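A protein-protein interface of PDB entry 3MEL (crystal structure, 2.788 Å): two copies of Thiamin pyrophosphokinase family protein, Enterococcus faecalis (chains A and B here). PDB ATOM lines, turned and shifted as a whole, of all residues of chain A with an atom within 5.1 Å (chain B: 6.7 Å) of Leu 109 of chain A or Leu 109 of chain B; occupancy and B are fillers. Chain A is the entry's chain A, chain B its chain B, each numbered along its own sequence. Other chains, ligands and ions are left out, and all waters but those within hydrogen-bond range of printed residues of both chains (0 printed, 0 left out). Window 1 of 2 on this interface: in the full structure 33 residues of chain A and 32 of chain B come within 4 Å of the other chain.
The backbone carbonyl oxygen of Asp 107 of chain A is in hydrogen-bond range of the side-chain hydroxyl of Ser 186 of chain B, 2.9 Å away.
The guanidinium group (NH1) of Arg 105 of chain A is in salt-bridge range of the side-chain carboxylate (OD1) of Asp 107 of chain A (2.7 Å).
Leu 109 of chain A touches Leu 109 of chain B (CD2 to CD1, 3.9 Å).
Leu 110 of chain A touches Leu 113 of chain B (CD2 to CD2, 3.7 Å).
N of Ala 111 of chain A touches CB of Ser 186 of chain B, 3.8 Å away.
Leu 113 of chain A touches Leu 110 of chain B (CD2 to CD1, 3.8 Å).
Of chain B, only Leu 109 (3.9 Å) comes within 4 Å of Leu 109 of chain A.
Leu 109 of chain B touches just one residue of chain A: Leu 109 (3.9 Å).
Of the printed residues of chain A, Leu 110 of chain B touches Leu 113 (3.8 Å).
Printed residues of chain B within 4 Å of Ala 111 of chain A: Ser 186 (3.8 Å).
Of the printed residues of chain B, Leu 110 of chain A touches Leu 113.
Printed residues of chain A within 4 Å of Ser 186 of chain B: Asp 107 (2.9 Å) and Ala 111 (3.8 Å).
Printed residues of chain A within 4 Å of Leu 113 of chain B: Leu 110.
The nearest residue of chain A that does not touch Leu 109 of chain B is Ile 106 of chain A (4.7 Å).
The nearest printed residue of chain A that does not touch Ser 186 of chain B is Leu 110 of chain A (4.2 Å).
Of the 18 printed residues of chain B, 4 touch a printed residue of chain A.
Printed residues of chain B that touch a printed residue of chain A: Leu 109, Leu 110, Leu 113 and Ser 186.
Along chain B the printed residues that touch a printed residue of chain A span positions 109 to 186.
Hydrophobic or aromatic side chains of chain A that line the printed part of chain B: Leu 109, Leu 110 and Leu 113.
Along chain A the printed residues that touch a printed residue of chain B span positions 107 to 113.
Among the printed residues, no Asp or Glu carboxylate lies within 4 Å of a Lys or Arg side-chain nitrogen of the other chain.
Leu 109 of chain B touches its own counterpart, Leu 109 of chain A.
Leu 110 of chain A touches Leu 113 of chain B, and with the chains exchanged Leu 113 of chain A touches Leu 110 of chain B.
9 positions are printed for both chains.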
ATOM      1  N   ARG A 105       2.900   0.499 -22.744  1.00  0.00           N
ATOM      2  CA  ARG A 105       2.103  -0.288 -23.674  1.00  0.00           C
ATOM      3  C   ARG A 105       1.089  -1.136 -22.927  1.00  0.00           C
ATOM      4  O   ARG A 105       1.446  -1.937 -22.068  1.00  0.00           O
ATOM      5  CB  ARG A 105       3.013  -1.137 -24.568  1.00  0.00           C
ATOM      6  CG  ARG A 105       3.126  -0.571 -25.978  1.00  0.00           C
ATOM      7  CD  ARG A 105       4.502  -0.693 -26.591  1.00  0.00           C
ATOM      8  NE  ARG A 105       4.854  -1.999 -27.167  1.00  0.00           N
ATOM      9  CZ  ARG A 105       4.026  -3.002 -27.455  1.00  0.00           C
ATOM     10  NH1 ARG A 105       2.726  -2.907 -27.234  1.00  0.00           N
ATOM     11  NH2 ARG A 105       4.515  -4.121 -27.969  1.00  0.00           N
ATOM     12  N   ILE A 106      -0.189  -0.962 -23.258  1.00  0.00           N
ATOM     13  CA  ILE A 106      -1.229  -1.533 -22.417  1.00  0.00           C
ATOM     14  C   ILE A 106      -1.420  -3.035 -22.624  1.00  0.00           C
ATOM     15  O   ILE A 106      -1.823  -3.730 -21.701  1.00  0.00           O
ATOM     16  CB  ILE A 106      -2.554  -0.710 -22.443  1.00  0.00           C
ATOM     17  CG1 ILE A 106      -2.274   0.779 -22.198  1.00  0.00           C
ATOM     18  CG2 ILE A 106      -3.542  -1.220 -21.384  1.00  0.00           C
ATOM     19  CD1 ILE A 106      -3.515   1.631 -22.003  1.00  0.00           C
ATOM     20  N   ASP A 107      -1.099  -3.546 -23.810  1.00  0.00           N
ATOM     21  CA  ASP A 107      -1.022  -4.995 -23.988  1.00  0.00           C
ATOM     22  C   ASP A 107      -0.015  -5.617 -23.010  1.00  0.00           C
ATOM     23  O   ASP A 107      -0.286  -6.640 -22.395  1.00  0.00           O
ATOM     24  CB  ASP A 107      -0.701  -5.395 -25.439  1.00  0.00           C
ATOM     25  CG  ASP A 107       0.337  -4.499 -26.095  1.00  0.00           C
ATOM     26  OD1 ASP A 107       0.870  -3.589 -25.432  1.00  0.00           O
ATOM     27  OD2 ASP A 107       0.613  -4.706 -27.293  1.00  0.00           O
ATOM     28  N   HIS A 108       1.147  -4.991 -22.866  1.00  0.00           N
ATOM     29  CA  HIS A 108       2.112  -5.434 -21.883  1.00  0.00           C
ATOM     30  C   HIS A 108       1.650  -5.151 -20.459  1.00  0.00           C
ATOM     31  O   HIS A 108       1.876  -5.951 -19.556  1.00  0.00           O
ATOM     32  CB  HIS A 108       3.463  -4.793 -22.131  1.00  0.00           C
ATOM     33  CG  HIS A 108       4.234  -5.450 -23.219  1.00  0.00           C
ATOM     34  ND1 HIS A 108       5.031  -4.749 -24.094  1.00  0.00           N
ATOM     35  CD2 HIS A 108       4.326  -6.751 -23.580  1.00  0.00           C
ATOM     36  CE1 HIS A 108       5.583  -5.592 -24.950  1.00  0.00           C
ATOM     37  NE2 HIS A 108       5.172  -6.814 -24.658  1.00  0.00           N
ATOM     38  N   LEU A 109       1.006  -4.020 -20.230  1.00  0.00           N
ATOM     39  CA  LEU A 109       0.479  -3.826 -18.892  1.00  0.00           C
ATOM     40  C   LEU A 109      -0.398  -5.042 -18.507  1.00  0.00           C
ATOM     41  O   LEU A 109      -0.127  -5.704 -17.507  1.00  0.00           O
ATOM     42  CB  LEU A 109      -0.261  -2.493 -18.754  1.00  0.00           C
ATOM     43  CG  LEU A 109      -1.039  -2.339 -17.447  1.00  0.00           C
ATOM     44  CD1 LEU A 109      -0.073  -2.180 -16.315  1.00  0.00           C
ATOM     45  CD2 LEU A 109      -1.984  -1.166 -17.503  1.00  0.00           C
ATOM     46  N   LEU A 110      -1.413  -5.357 -19.316  1.00  0.00           N
ATOM     47  CA  LEU A 110      -2.301  -6.499 -19.051  1.00  0.00           C
ATOM     48  C   LEU A 110      -1.618  -7.884 -19.147  1.00  0.00           C
ATOM     49  O   LEU A 110      -2.024  -8.861 -18.500  1.00  0.00           O
ATOM     50  CB  LEU A 110      -3.492  -6.448 -20.004  1.00  0.00           C
ATOM     51  CG  LEU A 110      -4.328  -5.173 -19.945  1.00  0.00           C
ATOM     52  CD1 LEU A 110      -5.314  -5.140 -21.102  1.00  0.00           C
ATOM     53  CD2 LEU A 110      -5.055  -5.074 -18.612  1.00  0.00           C
ATOM     54  N   ALA A 111      -0.587  -7.965 -19.974  1.00  0.00           N
ATOM     55  CA  ALA A 111       0.245  -9.154 -20.028  1.00  0.00           C
ATOM     56  C   ALA A 111       0.774  -9.424 -18.631  1.00  0.00           C
ATOM     57  O   ALA A 111       0.706 -10.547 -18.142  1.00  0.00           O
ATOM     58  CB  ALA A 111       1.391  -8.937 -20.999  1.00  0.00           C
ATOM     59  N   ASN A 112       1.273  -8.368 -17.989  1.00  0.00           N
ATOM     60  CA  ASN A 112       1.835  -8.438 -16.653  1.00  0.00           C
ATOM     61  C   ASN A 112       0.770  -8.680 -15.576  1.00  0.00           C
ATOM     62  O   ASN A 112       0.873  -9.590 -14.769  1.00  0.00           O
ATOM     63  CB  ASN A 112       2.620  -7.154 -16.343  1.00  0.00           C
ATOM     64  CG  ASN A 112       3.973  -7.073 -17.067  1.00  0.00           C
ATOM     65  OD1 ASN A 112       4.544  -8.083 -17.474  1.00  0.00           O
ATOM     66  ND2 ASN A 112       4.496  -5.862 -17.204  1.00  0.00           N
ATOM     67  N   LEU A 113      -0.262  -7.856 -15.582  1.00  0.00           N
ATOM     68  CA  LEU A 113      -1.356  -7.917 -14.623  1.00  0.00           C
ATOM     69  C   LEU A 113      -2.117  -9.249 -14.539  1.00  0.00           C
ATOM     70  O   LEU A 113      -2.863  -9.471 -13.604  1.00  0.00           O
ATOM     71  CB  LEU A 113      -2.344  -6.816 -14.992  1.00  0.00           C
ATOM     72  CG  LEU A 113      -3.518  -6.550 -14.069  1.00  0.00           C
ATOM     73  CD1 LEU A 113      -2.985  -6.136 -12.718  1.00  0.00           C
ATOM     74  CD2 LEU A 113      -4.384  -5.465 -14.665  1.00  0.00           C
ATOM     75  N   ALA B 101      -7.460   9.076 -19.145  1.00  0.00           N
ATOM     76  CA  ALA B 101      -7.883   8.101 -18.134  1.00  0.00           C
ATOM     77  C   ALA B 101      -6.807   7.061 -17.800  1.00  0.00           C
ATOM     78  O   ALA B 101      -7.096   6.051 -17.157  1.00  0.00           O
ATOM     79  CB  ALA B 101      -9.154   7.404 -18.565  1.00  0.00           C
ATOM     80  N   THR B 102      -5.573   7.326 -18.224  1.00  0.00           N
ATOM     81  CA  THR B 102      -4.456   6.396 -18.072  1.00  0.00           C
ATOM     82  C   THR B 102      -3.201   7.080 -17.487  1.00  0.00           C
ATOM     83  O   THR B 102      -3.261   8.190 -16.939  1.00  0.00           O
ATOM     84  CB  THR B 102      -4.084   5.839 -19.439  1.00  0.00           C
ATOM     85  OG1 THR B 102      -4.005   6.935 -20.359  1.00  0.00           O
ATOM     86  CG2 THR B 102      -5.145   4.845 -19.929  1.00  0.00           C
ATOM     87  N   GLY B 103      -2.059   6.416 -17.611  1.00  0.00           N
ATOM     88  CA  GLY B 103      -0.788   7.034 -17.260  1.00  0.00           C
ATOM     89  C   GLY B 103      -0.493   7.331 -15.788  1.00  0.00           C
ATOM     90  O   GLY B 103       0.598   7.820 -15.470  1.00  0.00           O
ATOM     91  N   GLY B 104      -1.444   7.051 -14.897  1.00  0.00           N
ATOM     92  CA  GLY B 104      -1.244   7.279 -13.477  1.00  0.00           C
ATOM     93  C   GLY B 104      -1.681   6.098 -12.628  1.00  0.00           C
ATOM     94  O   GLY B 104      -1.139   5.004 -12.757  1.00  0.00           O
ATOM     95  N   ARG B 105      -2.652   6.313 -11.750  1.00  0.00           N
ATOM     96  CA  ARG B 105      -3.194   5.233 -10.934  1.00  0.00           C
ATOM     97  C   ARG B 105      -3.812   4.138 -11.810  1.00  0.00           C
ATOM     98  O   ARG B 105      -4.497   4.403 -12.794  1.00  0.00           O
ATOM     99  CB  ARG B 105      -4.217   5.753  -9.913  1.00  0.00           C
ATOM    100  CG  ARG B 105      -3.629   6.398  -8.666  1.00  0.00           C
ATOM    101  CD  ARG B 105      -4.123   7.841  -8.435  1.00  0.00           C
ATOM    102  NE  ARG B 105      -5.411   8.002  -7.739  1.00  0.00           N
ATOM    103  CZ  ARG B 105      -6.195   7.021  -7.293  1.00  0.00           C
ATOM    104  NH1 ARG B 105      -5.858   5.751  -7.437  1.00  0.00           N
ATOM    105  NH2 ARG B 105      -7.338   7.311  -6.697  1.00  0.00           N
ATOM    106  N   ILE B 106      -3.561   2.899 -11.421  1.00  0.00           N
ATOM    107  CA  ILE B 106      -3.920   1.756 -12.220  1.00  0.00           C
ATOM    108  C   ILE B 106      -5.266   1.173 -11.818  1.00  0.00           C
ATOM    109  O   ILE B 106      -5.921   0.487 -12.624  1.00  0.00           O
ATOM    110  CB  ILE B 106      -2.822   0.700 -12.134  1.00  0.00           C
ATOM    111  CG1 ILE B 106      -1.589   1.204 -12.891  1.00  0.00           C
ATOM    112  CG2 ILE B 106      -3.305  -0.640 -12.676  1.00  0.00           C
ATOM    113  CD1 ILE B 106      -0.449   0.221 -12.935  1.00  0.00           C
ATOM    114  N   ASP B 107      -5.678   1.437 -10.579  1.00  0.00           N
ATOM    115  CA  ASP B 107      -7.001   1.019 -10.117  1.00  0.00           C
ATOM    116  C   ASP B 107      -8.050   1.874 -10.812  1.00  0.00           C
ATOM    117  O   ASP B 107      -9.217   1.519 -10.876  1.00  0.00           O
ATOM    118  CB  ASP B 107      -7.120   1.119  -8.590  1.00  0.00           C
ATOM    119  CG  ASP B 107      -6.989   2.546  -8.068  1.00  0.00           C
ATOM    120  OD1 ASP B 107      -6.279   3.365  -8.691  1.00  0.00           O
ATOM    121  OD2 ASP B 107      -7.589   2.842  -7.012  1.00  0.00           O
ATOM    122  N   HIS B 108      -7.603   3.004 -11.341  1.00  0.00           N
ATOM    123  CA  HIS B 108      -8.478   3.929 -12.025  1.00  0.00           C
ATOM    124  C   HIS B 108      -8.432   3.587 -13.497  1.00  0.00           C
ATOM    125  O   HIS B 108      -9.421   3.728 -14.189  1.00  0.00           O
ATOM    126  CB  HIS B 108      -8.014   5.362 -11.798  1.00  0.00           C
ATOM    127  CG  HIS B 108      -9.063   6.388 -12.066  1.00  0.00           C
ATOM    128  ND1 HIS B 108      -9.450   7.320 -11.123  1.00  0.00           N
ATOM    129  CD2 HIS B 108      -9.807   6.640 -13.171  1.00  0.00           C
ATOM    130  CE1 HIS B 108     -10.387   8.100 -11.639  1.00  0.00           C
ATOM    131  NE2 HIS B 108     -10.623   7.710 -12.880  1.00  0.00           N
ATOM    132  N   LEU B 109      -7.284   3.127 -13.979  1.00  0.00           N
ATOM    133  CA  LEU B 109      -7.169   2.718 -15.372  1.00  0.00           C
ATOM    134  C   LEU B 109      -8.072   1.515 -15.615  1.00  0.00           C
ATOM    135  O   LEU B 109      -8.809   1.465 -16.615  1.00  0.00           O
ATOM    136  CB  LEU B 109      -5.717   2.384 -15.738  1.00  0.00           C
ATOM    137  CG  LEU B 109      -5.323   1.920 -17.150  1.00  0.00           C
ATOM    138  CD1 LEU B 109      -3.854   2.208 -17.379  1.00  0.00           C
ATOM    139  CD2 LEU B 109      -5.608   0.443 -17.395  1.00  0.00           C
ATOM    140  N   LEU B 110      -8.025   0.554 -14.695  1.00  0.00           N
ATOM    141  CA  LEU B 110      -8.866  -0.635 -14.797  1.00  0.00           C
ATOM    142  C   LEU B 110     -10.369  -0.311 -14.756  1.00  0.00           C
ATOM    143  O   LEU B 110     -11.165  -0.871 -15.510  1.00  0.00           O
ATOM    144  CB  LEU B 110      -8.508  -1.628 -13.692  1.00  0.00           C
ATOM    145  CG  LEU B 110      -7.123  -2.256 -13.800  1.00  0.00           C
ATOM    146  CD1 LEU B 110      -7.032  -3.422 -12.858  1.00  0.00           C
ATOM    147  CD2 LEU B 110      -6.945  -2.704 -15.231  1.00  0.00           C
ATOM    148  N   ALA B 111     -10.755   0.594 -13.871  1.00  0.00           N
ATOM    149  CA  ALA B 111     -12.144   0.995 -13.787  1.00  0.00           C
ATOM    150  C   ALA B 111     -12.643   1.547 -15.127  1.00  0.00           C
ATOM    151  O   ALA B 111     -13.838   1.499 -15.408  1.00  0.00           O
ATOM    152  CB  ALA B 111     -12.325   2.012 -12.677  1.00  0.00           C
ATOM    153  N   ASN B 112     -11.722   2.071 -15.932  1.00  0.00           N
ATOM    154  CA  ASN B 112     -12.026   2.607 -17.253  1.00  0.00           C
ATOM    155  C   ASN B 112     -11.947   1.512 -18.317  1.00  0.00           C
ATOM    156  O   ASN B 112     -12.694   1.510 -19.292  1.00  0.00           O
ATOM    157  CB  ASN B 112     -11.047   3.727 -17.607  1.00  0.00           C
ATOM    158  CG  ASN B 112     -11.502   5.094 -17.118  1.00  0.00           C
ATOM    159  OD1 ASN B 112     -11.306   5.470 -15.962  1.00  0.00           O
ATOM    160  ND2 ASN B 112     -12.102   5.853 -18.008  1.00  0.00           N
ATOM    161  N   LEU B 113     -11.021   0.578 -18.135  1.00  0.00           N
ATOM    162  CA  LEU B 113     -10.859  -0.491 -19.100  1.00  0.00           C
ATOM    163  C   LEU B 113     -12.095  -1.375 -19.046  1.00  0.00           C
ATOM    164  O   LEU B 113     -12.487  -1.993 -20.042  1.00  0.00           O
ATOM    165  CB  LEU B 113      -9.589  -1.293 -18.817  1.00  0.00           C
ATOM    166  CG  LEU B 113      -9.334  -2.572 -19.630  1.00  0.00           C
ATOM    167  CD1 LEU B 113      -8.840  -2.260 -21.044  1.00  0.00           C
ATOM    168  CD2 LEU B 113      -8.372  -3.514 -18.910  1.00  0.00           C
ATOM    169  N   TRP B 114     -12.733  -1.398 -17.888  1.00  0.00           N
ATOM    170  CA  TRP B 114     -13.834  -2.316 -17.652  1.00  0.00           C
ATOM    171  C   TRP B 114     -15.221  -1.703 -17.794  1.00  0.00           C
ATOM    172  O   TRP B 114     -16.204  -2.322 -17.438  1.00  0.00           O
ATOM    173  CB  TRP B 114     -13.685  -2.952 -16.278  1.00  0.00           C
ATOM    174  CG  TRP B 114     -12.514  -3.844 -16.179  1.00  0.00           C
ATOM    175  CD1 TRP B 114     -11.901  -4.508 -17.201  1.00  0.00           C
ATOM    176  CD2 TRP B 114     -11.806  -4.205 -14.979  1.00  0.00           C
ATOM    177  NE1 TRP B 114     -10.856  -5.257 -16.714  1.00  0.00           N
ATOM    178  CE2 TRP B 114     -10.781  -5.088 -15.353  1.00  0.00           C
ATOM    179  CE3 TRP B 114     -11.947  -3.868 -13.626  1.00  0.00           C
ATOM    180  CZ2 TRP B 114      -9.908  -5.639 -14.431  1.00  0.00           C
ATOM    181  CZ3 TRP B 114     -11.079  -4.411 -12.717  1.00  0.00           C
ATOM    182  CH2 TRP B 114     -10.074  -5.286 -13.119  1.00  0.00           C
ATOM    183  N   LEU B 130     -11.009   3.893 -25.634  1.00  0.00           N
ATOM    184  CA  LEU B 130      -9.968   4.403 -24.716  1.00  0.00           C
ATOM    185  C   LEU B 130      -8.640   4.782 -25.388  1.00  0.00           C
ATOM    186  O   LEU B 130      -7.986   3.936 -25.984  1.00  0.00           O
ATOM    187  CB  LEU B 130      -9.665   3.345 -23.654  1.00  0.00           C
ATOM    188  CG  LEU B 130     -10.423   3.383 -22.331  1.00  0.00           C
ATOM    189  CD1 LEU B 130      -9.735   2.504 -21.311  1.00  0.00           C
ATOM    190  CD2 LEU B 130     -10.493   4.809 -21.825  1.00  0.00           C
ATOM    191  N   ASP B 132      -4.694   7.041 -25.557  1.00  0.00           N
ATOM    192  CA  ASP B 132      -3.605   7.855 -25.034  1.00  0.00           C
ATOM    193  C   ASP B 132      -2.463   7.870 -26.041  1.00  0.00           C
ATOM    194  O   ASP B 132      -2.531   7.175 -27.042  1.00  0.00           O
ATOM    195  CB  ASP B 132      -3.171   7.437 -23.613  1.00  0.00           C
ATOM    196  CG  ASP B 132      -2.437   6.090 -23.544  1.00  0.00           C
ATOM    197  OD1 ASP B 132      -2.206   5.628 -22.399  1.00  0.00           O
ATOM    198  OD2 ASP B 132      -2.065   5.495 -24.581  1.00  0.00           O
ATOM    199  N   ILE B 137      -7.557   1.520 -27.707  1.00  0.00           N
ATOM    200  CA  ILE B 137      -8.302   0.337 -27.303  1.00  0.00           C
ATOM    201  C   ILE B 137      -9.729   0.355 -27.806  1.00  0.00           C
ATOM    202  O   ILE B 137     -10.429   1.365 -27.681  1.00  0.00           O
ATOM    203  CB  ILE B 137      -8.373   0.240 -25.770  1.00  0.00           C
ATOM    204  CG1 ILE B 137      -6.966   0.113 -25.180  1.00  0.00           C
ATOM    205  CG2 ILE B 137      -9.295  -0.895 -25.336  1.00  0.00           C
ATOM    206  CD1 ILE B 137      -6.913   0.203 -23.681  1.00  0.00           C
ATOM    207  N   SER B 186      -3.269 -12.062 -22.742  1.00  0.00           N
ATOM    208  CA  SER B 186      -3.063 -10.895 -23.583  1.00  0.00           C
ATOM    209  C   SER B 186      -2.058 -11.155 -24.699  1.00  0.00           C
ATOM    210  O   SER B 186      -0.886 -10.809 -24.586  1.00  0.00           O
ATOM    211  CB  SER B 186      -2.613  -9.699 -22.748  1.00  0.00           C
ATOM    212  OG  SER B 186      -1.962  -8.728 -23.549  1.00  0.00           O
